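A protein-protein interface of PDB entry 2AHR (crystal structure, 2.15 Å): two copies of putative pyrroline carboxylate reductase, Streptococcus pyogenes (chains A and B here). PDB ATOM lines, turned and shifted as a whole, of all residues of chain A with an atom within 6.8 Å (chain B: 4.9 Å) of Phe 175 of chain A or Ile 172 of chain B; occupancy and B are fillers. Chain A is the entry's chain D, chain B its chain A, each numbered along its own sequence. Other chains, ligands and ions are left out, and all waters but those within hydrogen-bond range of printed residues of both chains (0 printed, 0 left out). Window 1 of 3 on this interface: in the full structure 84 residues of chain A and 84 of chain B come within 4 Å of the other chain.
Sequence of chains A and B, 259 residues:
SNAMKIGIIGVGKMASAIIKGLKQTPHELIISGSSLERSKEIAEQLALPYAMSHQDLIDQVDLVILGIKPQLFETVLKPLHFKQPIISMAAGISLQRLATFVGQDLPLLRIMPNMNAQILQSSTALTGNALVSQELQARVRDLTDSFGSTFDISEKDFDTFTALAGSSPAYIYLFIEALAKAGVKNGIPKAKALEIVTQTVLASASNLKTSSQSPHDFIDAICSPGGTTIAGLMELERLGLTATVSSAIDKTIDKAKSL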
ATOM      1  N   ALA A 170       3.600  20.863 -14.446  1.00  0.00           N
ATOM      2  CA  ALA A 170       3.187  19.471 -14.719  1.00  0.00           C
ATOM      3  C   ALA A 170       4.395  18.565 -14.845  1.00  0.00           C
ATOM      4  O   ALA A 170       4.367  17.434 -14.390  1.00  0.00           O
ATOM      5  CB  ALA A 170       2.341  19.388 -15.975  1.00  0.00           C
ATOM      6  N   TYR A 171       5.467  19.069 -15.451  1.00  0.00           N
ATOM      7  CA  TYR A 171       6.697  18.279 -15.610  1.00  0.00           C
ATOM      8  C   TYR A 171       7.436  18.106 -14.275  1.00  0.00           C
ATOM      9  O   TYR A 171       7.977  17.037 -13.996  1.00  0.00           O
ATOM     10  CB  TYR A 171       7.612  18.872 -16.701  1.00  0.00           C
ATOM     11  CG  TYR A 171       6.869  19.250 -17.965  1.00  0.00           C
ATOM     12  CD1 TYR A 171       5.689  18.574 -18.348  1.00  0.00           C
ATOM     13  CD2 TYR A 171       7.345  20.256 -18.804  1.00  0.00           C
ATOM     14  CE1 TYR A 171       4.996  18.928 -19.506  1.00  0.00           C
ATOM     15  CE2 TYR A 171       6.659  20.612 -19.984  1.00  0.00           C
ATOM     16  CZ  TYR A 171       5.488  19.943 -20.319  1.00  0.00           C
ATOM     17  OH  TYR A 171       4.795  20.284 -21.470  1.00  0.00           O
ATOM     18  N   ILE A 172       7.416  19.150 -13.448  1.00  0.00           N
ATOM     19  CA  ILE A 172       7.923  19.102 -12.094  1.00  0.00           C
ATOM     20  C   ILE A 172       7.173  18.076 -11.243  1.00  0.00           C
ATOM     21  O   ILE A 172       7.793  17.306 -10.507  1.00  0.00           O
ATOM     22  CB  ILE A 172       7.828  20.495 -11.435  1.00  0.00           C
ATOM     23  CG1 ILE A 172       8.911  21.421 -12.006  1.00  0.00           C
ATOM     24  CG2 ILE A 172       7.968  20.399  -9.932  1.00  0.00           C
ATOM     25  CD1 ILE A 172       8.473  22.876 -12.188  1.00  0.00           C
ATOM     26  N   TYR A 173       5.848  18.041 -11.341  1.00  0.00           N
ATOM     27  CA  TYR A 173       5.068  17.032 -10.611  1.00  0.00           C
ATOM     28  C   TYR A 173       5.260  15.601 -11.129  1.00  0.00           C
ATOM     29  O   TYR A 173       5.208  14.647 -10.357  1.00  0.00           O
ATOM     30  CB  TYR A 173       3.577  17.399 -10.626  1.00  0.00           C
ATOM     31  CG  TYR A 173       3.248  18.714  -9.922  1.00  0.00           C
ATOM     32  CD1 TYR A 173       3.792  19.013  -8.654  1.00  0.00           C
ATOM     33  CD2 TYR A 173       2.387  19.657 -10.522  1.00  0.00           C
ATOM     34  CE1 TYR A 173       3.503  20.246  -8.007  1.00  0.00           C
ATOM     35  CE2 TYR A 173       2.095  20.884  -9.884  1.00  0.00           C
ATOM     36  CZ  TYR A 173       2.652  21.157  -8.631  1.00  0.00           C
ATOM     37  OH  TYR A 173       2.352  22.350  -8.004  1.00  0.00           O
ATOM     38  N   LEU A 174       5.452  15.422 -12.428  1.00  0.00           N
ATOM     39  CA  LEU A 174       5.712  14.048 -12.935  1.00  0.00           C
ATOM     40  C   LEU A 174       7.056  13.562 -12.387  1.00  0.00           C
ATOM     41  O   LEU A 174       7.206  12.400 -12.009  1.00  0.00           O
ATOM     42  CB  LEU A 174       5.678  13.997 -14.469  1.00  0.00           C
ATOM     43  CG  LEU A 174       5.692  12.586 -15.094  1.00  0.00           C
ATOM     44  CD1 LEU A 174       4.313  11.925 -14.940  1.00  0.00           C
ATOM     45  CD2 LEU A 174       6.088  12.646 -16.591  1.00  0.00           C
ATOM     46  N   PHE A 175       8.012  14.479 -12.285  1.00  0.00           N
ATOM     47  CA  PHE A 175       9.340  14.173 -11.742  1.00  0.00           C
ATOM     48  C   PHE A 175       9.250  13.789 -10.270  1.00  0.00           C
ATOM     49  O   PHE A 175       9.799  12.768  -9.853  1.00  0.00           O
ATOM     50  CB  PHE A 175      10.251  15.395 -11.951  1.00  0.00           C
ATOM     51  CG  PHE A 175      11.681  15.191 -11.510  1.00  0.00           C
ATOM     52  CD1 PHE A 175      12.567  14.446 -12.280  1.00  0.00           C
ATOM     53  CD2 PHE A 175      12.136  15.763 -10.328  1.00  0.00           C
ATOM     54  CE1 PHE A 175      13.884  14.266 -11.880  1.00  0.00           C
ATOM     55  CE2 PHE A 175      13.466  15.596  -9.921  1.00  0.00           C
ATOM     56  CZ  PHE A 175      14.338  14.844 -10.709  1.00  0.00           C
ATOM     57  N   ILE A 176       8.600  14.651  -9.464  1.00  0.00           N
ATOM     58  CA  ILE A 176       8.333  14.369  -8.059  1.00  0.00           C
ATOM     59  C   ILE A 176       7.614  13.013  -7.878  1.00  0.00           C
ATOM     60  O   ILE A 176       7.973  12.198  -7.018  1.00  0.00           O
ATOM     61  CB  ILE A 176       7.481  15.499  -7.446  1.00  0.00           C
ATOM     62  CG1 ILE A 176       8.331  16.765  -7.255  1.00  0.00           C
ATOM     63  CG2 ILE A 176       6.817  15.064  -6.124  1.00  0.00           C
ATOM     64  CD1 ILE A 176       7.503  18.032  -6.897  1.00  0.00           C
ATOM     65  N   GLU A 177       6.585  12.792  -8.675  1.00  0.00           N
ATOM     66  CA  GLU A 177       5.833  11.541  -8.637  1.00  0.00           C
ATOM     67  C   GLU A 177       6.747  10.351  -8.923  1.00  0.00           C
ATOM     68  O   GLU A 177       6.617   9.305  -8.283  1.00  0.00           O
ATOM     69  CB  GLU A 177       4.667  11.608  -9.636  1.00  0.00           C
ATOM     70  CG  GLU A 177       3.789  10.357  -9.738  1.00  0.00           C
ATOM     71  CD  GLU A 177       3.008  10.047  -8.478  1.00  0.00           C
ATOM     72  OE1 GLU A 177       2.855  10.927  -7.598  1.00  0.00           O
ATOM     73  OE2 GLU A 177       2.555   8.901  -8.365  1.00  0.00           O
ATOM     74  N   ALA A 178       7.687  10.521  -9.857  1.00  0.00           N
ATOM     75  CA  ALA A 178       8.605   9.421 -10.238  1.00  0.00           C
ATOM     76  C   ALA A 178       9.540   9.088  -9.072  1.00  0.00           C
ATOM     77  O   ALA A 178       9.830   7.916  -8.815  1.00  0.00           O
ATOM     78  CB  ALA A 178       9.399   9.802 -11.453  1.00  0.00           C
ATOM     79  N   LEU A 179       9.980  10.129  -8.352  1.00  0.00           N
ATOM     80  CA  LEU A 179      10.841   9.969  -7.190  1.00  0.00           C
ATOM     81  C   LEU A 179      10.083   9.271  -6.068  1.00  0.00           C
ATOM     82  O   LEU A 179      10.616   8.372  -5.430  1.00  0.00           O
ATOM     83  CB  LEU A 179      11.343  11.339  -6.686  1.00  0.00           C
ATOM     84  CG  LEU A 179      12.460  12.002  -7.506  1.00  0.00           C
ATOM     85  CD1 LEU A 179      12.745  13.395  -6.983  1.00  0.00           C
ATOM     86  CD2 LEU A 179      13.746  11.163  -7.480  1.00  0.00           C
ATOM     87  N   ALA A 180       8.844   9.696  -5.837  1.00  0.00           N
ATOM     88  CA  ALA A 180       7.964   9.074  -4.842  1.00  0.00           C
ATOM     89  C   ALA A 180       7.631   7.612  -5.151  1.00  0.00           C
ATOM     90  O   ALA A 180       7.645   6.784  -4.253  1.00  0.00           O
ATOM     91  CB  ALA A 180       6.708   9.879  -4.675  1.00  0.00           C
ATOM     92  N   VAL A 197      10.318  13.819  -0.537  1.00  0.00           N
ATOM     93  CA  VAL A 197      10.845  14.401  -1.771  1.00  0.00           C
ATOM     94  C   VAL A 197      10.340  15.808  -2.015  1.00  0.00           C
ATOM     95  O   VAL A 197      11.095  16.632  -2.493  1.00  0.00           O
ATOM     96  CB  VAL A 197      10.850  13.492  -3.089  1.00  0.00           C
ATOM     97  CG1 VAL A 197      10.850  12.023  -2.806  1.00  0.00           C
ATOM     98  CG2 VAL A 197       9.803  13.905  -4.088  1.00  0.00           C
ATOM     99  N   THR A 200      12.376  18.115   0.002  1.00  0.00           N
ATOM    100  CA  THR A 200      13.720  18.188  -0.583  1.00  0.00           C
ATOM    101  C   THR A 200      13.764  19.076  -1.842  1.00  0.00           C
ATOM    102  O   THR A 200      14.640  19.934  -1.963  1.00  0.00           O
ATOM    103  CB  THR A 200      14.311  16.774  -0.837  1.00  0.00           C
ATOM    104  OG1 THR A 200      14.355  16.068   0.406  1.00  0.00           O
ATOM    105  CG2 THR A 200      15.716  16.846  -1.389  1.00  0.00           C
ATOM    106  N   VAL A 201      12.825  18.877  -2.766  1.00  0.00           N
ATOM    107  CA  VAL A 201      12.695  19.745  -3.954  1.00  0.00           C
ATOM    108  C   VAL A 201      12.533  21.216  -3.535  1.00  0.00           C
ATOM    109  O   VAL A 201      13.185  22.129  -4.088  1.00  0.00           O
ATOM    110  CB  VAL A 201      11.491  19.317  -4.803  1.00  0.00           C
ATOM    111  CG1 VAL A 201      11.131  20.381  -5.855  1.00  0.00           C
ATOM    112  CG2 VAL A 201      11.743  17.937  -5.484  1.00  0.00           C
ATOM    113  N   LEU A 202      11.667  21.449  -2.556  1.00  0.00           N
ATOM    114  CA  LEU A 202      11.411  22.806  -2.085  1.00  0.00           C
ATOM    115  C   LEU A 202      12.684  23.449  -1.523  1.00  0.00           C
ATOM    116  O   LEU A 202      13.019  24.582  -1.879  1.00  0.00           O
ATOM    117  CB  LEU A 202      10.276  22.790  -1.052  1.00  0.00           C
ATOM    118  CG  LEU A 202       9.644  24.101  -0.588  1.00  0.00           C
ATOM    119  CD1 LEU A 202       8.989  24.831  -1.724  1.00  0.00           C
ATOM    120  CD2 LEU A 202       8.588  23.802   0.473  1.00  0.00           C
ATOM    121  N   SER A 204      15.943  22.395  -1.953  1.00  0.00           N
ATOM    122  CA  SER A 204      16.938  22.435  -3.025  1.00  0.00           C
ATOM    123  C   SER A 204      16.775  23.677  -3.890  1.00  0.00           C
ATOM    124  O   SER A 204      17.748  24.410  -4.133  1.00  0.00           O
ATOM    125  CB  SER A 204      16.810  21.197  -3.944  1.00  0.00           C
ATOM    126  OG  SER A 204      17.152  20.028  -3.243  1.00  0.00           O
ATOM    127  N   ALA A 205      15.552  23.893  -4.382  1.00  0.00           N
ATOM    128  CA  ALA A 205      15.292  25.076  -5.198  1.00  0.00           C
ATOM    129  C   ALA A 205      15.536  26.385  -4.403  1.00  0.00           C
ATOM    130  O   ALA A 205      16.017  27.356  -4.964  1.00  0.00           O
ATOM    131  CB  ALA A 205      13.877  25.042  -5.800  1.00  0.00           C
ATOM    132  N   PRO A 215      23.601  25.213 -10.785  1.00  0.00           N
ATOM    133  CA  PRO A 215      23.167  23.817 -10.535  1.00  0.00           C
ATOM    134  C   PRO A 215      24.288  22.769 -10.649  1.00  0.00           C
ATOM    135  O   PRO A 215      24.385  21.863  -9.813  1.00  0.00           O
ATOM    136  CB  PRO A 215      22.099  23.596 -11.609  1.00  0.00           C
ATOM    137  CG  PRO A 215      21.557  24.992 -11.860  1.00  0.00           C
ATOM    138  CD  PRO A 215      22.731  25.902 -11.762  1.00  0.00           C
ATOM    139  N   ILE A 219      25.819  20.116  -7.975  1.00  0.00           N
ATOM    140  CA  ILE A 219      26.039  18.699  -8.304  1.00  0.00           C
ATOM    141  C   ILE A 219      27.442  18.257  -7.889  1.00  0.00           C
ATOM    142  O   ILE A 219      27.589  17.226  -7.234  1.00  0.00           O
ATOM    143  CB  ILE A 219      25.729  18.419  -9.767  1.00  0.00           C
ATOM    144  CG1 ILE A 219      24.207  18.580  -9.989  1.00  0.00           C
ATOM    145  CG2 ILE A 219      26.237  17.005 -10.189  1.00  0.00           C
ATOM    146  CD1 ILE A 219      23.780  18.516 -11.451  1.00  0.00           C
ATOM    147  N   LEU A 236      21.073   8.622 -14.787  1.00  0.00           N
ATOM    148  CA  LEU A 236      20.375   9.716 -15.495  1.00  0.00           C
ATOM    149  C   LEU A 236      21.001  10.112 -16.846  1.00  0.00           C
ATOM    150  O   LEU A 236      20.285  10.377 -17.809  1.00  0.00           O
ATOM    151  CB  LEU A 236      20.317  10.972 -14.599  1.00  0.00           C
ATOM    152  CG  LEU A 236      19.468  10.816 -13.333  1.00  0.00           C
ATOM    153  CD1 LEU A 236      19.508  12.064 -12.485  1.00  0.00           C
ATOM    154  CD2 LEU A 236      18.008  10.425 -13.690  1.00  0.00           C
ATOM    155  N   LEU A 241      18.225  11.766 -19.158  1.00  0.00           N
ATOM    156  CA  LEU A 241      17.288  12.662 -18.472  1.00  0.00           C
ATOM    157  C   LEU A 241      17.264  14.026 -19.165  1.00  0.00           C
ATOM    158  O   LEU A 241      16.185  14.545 -19.499  1.00  0.00           O
ATOM    159  CB  LEU A 241      17.617  12.821 -16.981  1.00  0.00           C
ATOM    160  CG  LEU A 241      16.813  13.930 -16.279  1.00  0.00           C
ATOM    161  CD1 LEU A 241      15.401  13.465 -16.060  1.00  0.00           C
ATOM    162  CD2 LEU A 241      17.381  14.302 -14.985  1.00  0.00           C
ATOM    163  N   VAL A 245      13.982  15.854 -21.073  1.00  0.00           N
ATOM    164  CA  VAL A 245      13.341  17.128 -20.653  1.00  0.00           C
ATOM    165  C   VAL A 245      13.343  18.132 -21.805  1.00  0.00           C
ATOM    166  O   VAL A 245      12.332  18.787 -22.094  1.00  0.00           O
ATOM    167  CB  VAL A 245      14.082  17.715 -19.429  1.00  0.00           C
ATOM    168  CG1 VAL A 245      13.506  19.089 -18.996  1.00  0.00           C
ATOM    169  CG2 VAL A 245      14.032  16.742 -18.262  1.00  0.00           C
ATOM    170  N   SER B 168      19.015  12.983  -3.967  1.00  0.00           N
ATOM    171  CA  SER B 168      18.078  13.610  -4.896  1.00  0.00           C
ATOM    172  C   SER B 168      18.310  15.097  -5.225  1.00  0.00           C
ATOM    173  O   SER B 168      17.926  15.536  -6.292  1.00  0.00           O
ATOM    174  CB  SER B 168      16.626  13.359  -4.463  1.00  0.00           C
ATOM    175  OG  SER B 168      16.322  14.070  -3.266  1.00  0.00           O
ATOM    176  N   PRO B 169      18.873  15.904  -4.288  1.00  0.00           N
ATOM    177  CA  PRO B 169      19.162  17.292  -4.693  1.00  0.00           C
ATOM    178  C   PRO B 169      19.958  17.375  -5.996  1.00  0.00           C
ATOM    179  O   PRO B 169      19.710  18.264  -6.795  1.00  0.00           O
ATOM    180  CB  PRO B 169      19.976  17.842  -3.525  1.00  0.00           C
ATOM    181  CG  PRO B 169      19.425  17.123  -2.344  1.00  0.00           C
ATOM    182  CD  PRO B 169      19.188  15.683  -2.860  1.00  0.00           C
ATOM    183  N   ALA B 170      20.895  16.459  -6.210  1.00  0.00           N
ATOM    184  CA  ALA B 170      21.675  16.443  -7.453  1.00  0.00           C
ATOM    185  C   ALA B 170      20.799  16.133  -8.667  1.00  0.00           C
ATOM    186  O   ALA B 170      21.010  16.696  -9.756  1.00  0.00           O
ATOM    187  CB  ALA B 170      22.824  15.437  -7.350  1.00  0.00           C
ATOM    188  N   TYR B 171      19.820  15.237  -8.485  1.00  0.00           N
ATOM    189  CA  TYR B 171      18.912  14.863  -9.574  1.00  0.00           C
ATOM    190  C   TYR B 171      17.960  15.993  -9.861  1.00  0.00           C
ATOM    191  O   TYR B 171      17.688  16.290 -11.016  1.00  0.00           O
ATOM    192  CB  TYR B 171      18.154  13.560  -9.272  1.00  0.00           C
ATOM    193  CG  TYR B 171      19.074  12.465  -8.766  1.00  0.00           C
ATOM    194  CD1 TYR B 171      20.408  12.411  -9.170  1.00  0.00           C
ATOM    195  CD2 TYR B 171      18.612  11.476  -7.906  1.00  0.00           C
ATOM    196  CE1 TYR B 171      21.272  11.412  -8.722  1.00  0.00           C
ATOM    197  CE2 TYR B 171      19.464  10.464  -7.445  1.00  0.00           C
ATOM    198  CZ  TYR B 171      20.797  10.449  -7.859  1.00  0.00           C
ATOM    199  OH  TYR B 171      21.656   9.472  -7.411  1.00  0.00           O
ATOM    200  N   ILE B 172      17.462  16.619  -8.795  1.00  0.00           N
ATOM    201  CA  ILE B 172      16.676  17.828  -8.907  1.00  0.00           C
ATOM    202  C   ILE B 172      17.438  18.910  -9.671  1.00  0.00           C
ATOM    203  O   ILE B 172      16.872  19.538 -10.569  1.00  0.00           O
ATOM    204  CB  ILE B 172      16.252  18.341  -7.517  1.00  0.00           C
ATOM    205  CG1 ILE B 172      15.305  17.329  -6.851  1.00  0.00           C
ATOM    206  CG2 ILE B 172      15.609  19.732  -7.602  1.00  0.00           C
ATOM    207  CD1 ILE B 172      15.368  17.316  -5.326  1.00  0.00           C
ATOM    208  N   TYR B 173      18.709  19.116  -9.333  1.00  0.00           N
ATOM    209  CA  TYR B 173      19.504  20.142 -10.010  1.00  0.00           C
ATOM    210  C   TYR B 173      19.773  19.801 -11.486  1.00  0.00           C
ATOM    211  O   TYR B 173      19.783  20.681 -12.347  1.00  0.00           O
ATOM    212  CB  TYR B 173      20.811  20.453  -9.248  1.00  0.00           C
ATOM    213  CG  TYR B 173      20.591  21.110  -7.876  1.00  0.00           C
ATOM    214  CD1 TYR B 173      19.711  22.180  -7.715  1.00  0.00           C
ATOM    215  CD2 TYR B 173      21.272  20.656  -6.749  1.00  0.00           C
ATOM    216  CE1 TYR B 173      19.507  22.771  -6.465  1.00  0.00           C
ATOM    217  CE2 TYR B 173      21.066  21.238  -5.483  1.00  0.00           C
ATOM    218  CZ  TYR B 173      20.193  22.294  -5.352  1.00  0.00           C
ATOM    219  OH  TYR B 173      20.004  22.874  -4.114  1.00  0.00           O
ATOM    220  N   LEU B 174      20.000  18.523 -11.789  1.00  0.00           N
ATOM    221  CA  LEU B 174      20.171  18.159 -13.198  1.00  0.00           C
ATOM    222  C   LEU B 174      18.865  18.450 -13.932  1.00  0.00           C
ATOM    223  O   LEU B 174      18.863  18.888 -15.075  1.00  0.00           O
ATOM    224  CB  LEU B 174      20.565  16.678 -13.360  1.00  0.00           C
ATOM    225  CG  LEU B 174      21.092  16.296 -14.750  1.00  0.00           C
ATOM    226  CD1 LEU B 174      22.501  16.867 -15.018  1.00  0.00           C
ATOM    227  CD2 LEU B 174      21.070  14.749 -14.970  1.00  0.00           C
ATOM    228  N   PHE B 175      17.743  18.221 -13.266  1.00  0.00           N
ATOM    229  CA  PHE B 175      16.447  18.428 -13.908  1.00  0.00           C
ATOM    230  C   PHE B 175      16.185  19.911 -14.218  1.00  0.00           C
ATOM    231  O   PHE B 175      15.766  20.289 -15.324  1.00  0.00           O
ATOM    232  CB  PHE B 175      15.374  17.848 -12.976  1.00  0.00           C
ATOM    233  CG  PHE B 175      13.960  18.017 -13.483  1.00  0.00           C
ATOM    234  CD1 PHE B 175      13.444  17.156 -14.457  1.00  0.00           C
ATOM    235  CD2 PHE B 175      13.143  19.022 -12.966  1.00  0.00           C
ATOM    236  CE1 PHE B 175      12.126  17.294 -14.915  1.00  0.00           C
ATOM    237  CE2 PHE B 175      11.843  19.167 -13.411  1.00  0.00           C
ATOM    238  CZ  PHE B 175      11.328  18.290 -14.391  1.00  0.00           C
ATOM    239  N   ILE B 176      16.411  20.752 -13.208  1.00  0.00           N
ATOM    240  CA  ILE B 176      16.322  22.193 -13.345  1.00  0.00           C
ATOM    241  C   ILE B 176      17.239  22.690 -14.461  1.00  0.00           C
ATOM    242  O   ILE B 176      16.830  23.479 -15.315  1.00  0.00           O
ATOM    243  CB  ILE B 176      16.675  22.874 -11.984  1.00  0.00           C
ATOM    244  CG1 ILE B 176      15.512  22.732 -11.006  1.00  0.00           C
ATOM    245  CG2 ILE B 176      17.074  24.352 -12.175  1.00  0.00           C
ATOM    246  CD1 ILE B 176      15.863  23.052  -9.558  1.00  0.00           C
ATOM    247  N   LEU B 241      10.583   9.531 -18.844  1.00  0.00           N
ATOM    248  CA  LEU B 241      10.991  10.291 -17.651  1.00  0.00           C
ATOM    249  C   LEU B 241      10.877   9.471 -16.364  1.00  0.00           C
ATOM    250  O   LEU B 241      11.822   9.396 -15.582  1.00  0.00           O
ATOM    251  CB  LEU B 241      10.222  11.602 -17.517  1.00  0.00           C
ATOM    252  CG  LEU B 241      10.643  12.272 -16.185  1.00  0.00           C
ATOM    253  CD1 LEU B 241      11.975  13.001 -16.383  1.00  0.00           C
ATOM    254  CD2 LEU B 241       9.614  13.179 -15.659  1.00  0.00           C
ATOM    255  N   VAL B 245      14.075   8.187 -13.854  1.00  0.00           N
ATOM    256  CA  VAL B 245      14.256   8.598 -12.454  1.00  0.00           C
ATOM    257  C   VAL B 245      14.310   7.377 -11.522  1.00  0.00           C
ATOM    258  O   VAL B 245      15.198   7.246 -10.674  1.00  0.00           O
ATOM    259  CB  VAL B 245      13.119   9.545 -12.059  1.00  0.00           C
ATOM    260  CG1 VAL B 245      13.129   9.820 -10.549  1.00  0.00           C
ATOM    261  CG2 VAL B 245      13.245  10.838 -12.881  1.00  0.00           C
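Tyr 171 of chain A touches Phe 175 of chain B, and with the chains exchanged Phe 175 of chain A touches Tyr 171 of chain B.
Ile 172 of chain A touches Phe 175 of chain B, and with the chains exchanged Phe 175 of chain A touches Ile 172 of chain B.
Leu 174 of chain A touches Leu 241 of chain B, and with the chains exchanged Leu 241 of chain A touches Leu 174 of chain B.
Phe 175 of chain A touches Leu 241 of chain B, but with the chains exchanged Leu 241 of chain A does not touch Phe 175 of chain B (4.3 Å).
Positions printed for both chains: 170, 171, 172, 173, 174, 175, 176, 241 and 245.
Of the 26 pairs that touch across the chains among the printed residues, 10 have their exchanged pair printed and touching as well.
The side-chain hydroxyl (OG) of Ser 204 of chain A sits at hydrogen-bond distance from the backbone carbonyl oxygen (O) of Thr 200 of chain A.
O of Leu 236 of chain A sits at hydrogen-bond distance from N of Leu 241 of chain A, at 2.8 Å.
Of the 11 printed residues of chain B, 10 touch a printed residue of chain A.
Hydrophobic or aromatic side chains of chain B within 4 Å of the printed part of chain A: Pro 169, Tyr 171, Ile 172, Tyr 173, Leu 174, Phe 175, Leu 241 and Val 245.
Hydrophobic or aromatic side chains of chain A within 4 Å of the printed part of chain B: Ile 172, Leu 174, Phe 175, Ala 178, Leu 179, Val 201, Pro 215, Ile 219, Leu 236, Leu 241 and Val 245.
Among the printed residues, 26 pairs touch across the chains.
Among the printed residues, no Asp or Glu carboxylate lies within 4 Å of a Lys or Arg side-chain nitrogen of the other chain.
The backbone carbonyl oxygen of Ser 204 of chain A is in hydrogen-bond range of the side-chain hydroxyl of Tyr 173 of chain B (2.7 Å).
Phe 175 of chain B touches Tyr 171 of chain A (CZ to O, 3.6 Å).
Ile 172 of chain A touches Phe 175 of chain B.
Leu 241 of chain B touches Phe 175 of chain A (CD2 to N, 3.95 Å).
CG of Pro 169 of chain B touches CG2 of Thr 200 of chain A, at 3.8 Å.
Val 201 of chain A touches Ile 172 of chain B (CG2 to CD1, 3.7 Å).
Ser 204 of chain A touches Pro 169 of chain B (OG to CB, 3.6 Å).
Tyr 173 of chain B touches Ile 219 of chain A (CB to CG1, 3.9 Å).
Ile 219 of chain A touches Leu 174 of chain B (CD1 to N, 3.8 Å).
Leu 236 of chain A touches Leu 174 of chain B (CB to CD2, 3.9 Å).
Val 245 of chain A touches Phe 175 of chain B.
Phe 175 of chain A touches just these residues of chain B: Tyr 171 (3.7 Å), Ile 172 (3.98 Å), Phe 175 (3.6 Å), Leu 241 (3.95 Å) and Val 245 (3.6 Å).
Of the printed residues of chain A, Ile 172 of chain B touches Phe 175 (3.98 Å), Thr 200 (3.98 Å), Val 201 (3.7 Å) and Ser 204 (3.9 Å).
Of the printed residues of chain A, Tyr 173 of chain B touches Ser 204 (2.7 Å), Pro 215 (3.8 Å) and Ile 219 (3.9 Å).
Of the printed residues of chain A, Ser 168 of chain B touches Thr 200 (3.4 Å).
Tyr 173 of chain A touches none of the printed residues of chain B.
Leu 202 of chain A touches none of the printed residues of chain B.
The nearest printed residue of chain B that does not touch Phe 175 of chain A is Ser 168 of chain B (5.7 Å).
The nearest printed residue of chain A that does not touch Ile 172 of chain B is Leu 179 of chain A (4.7 Å).
The nearest printed residue of chain B that does not touch Leu 241 of chain A is Phe 175 of chain B (4.3 Å).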
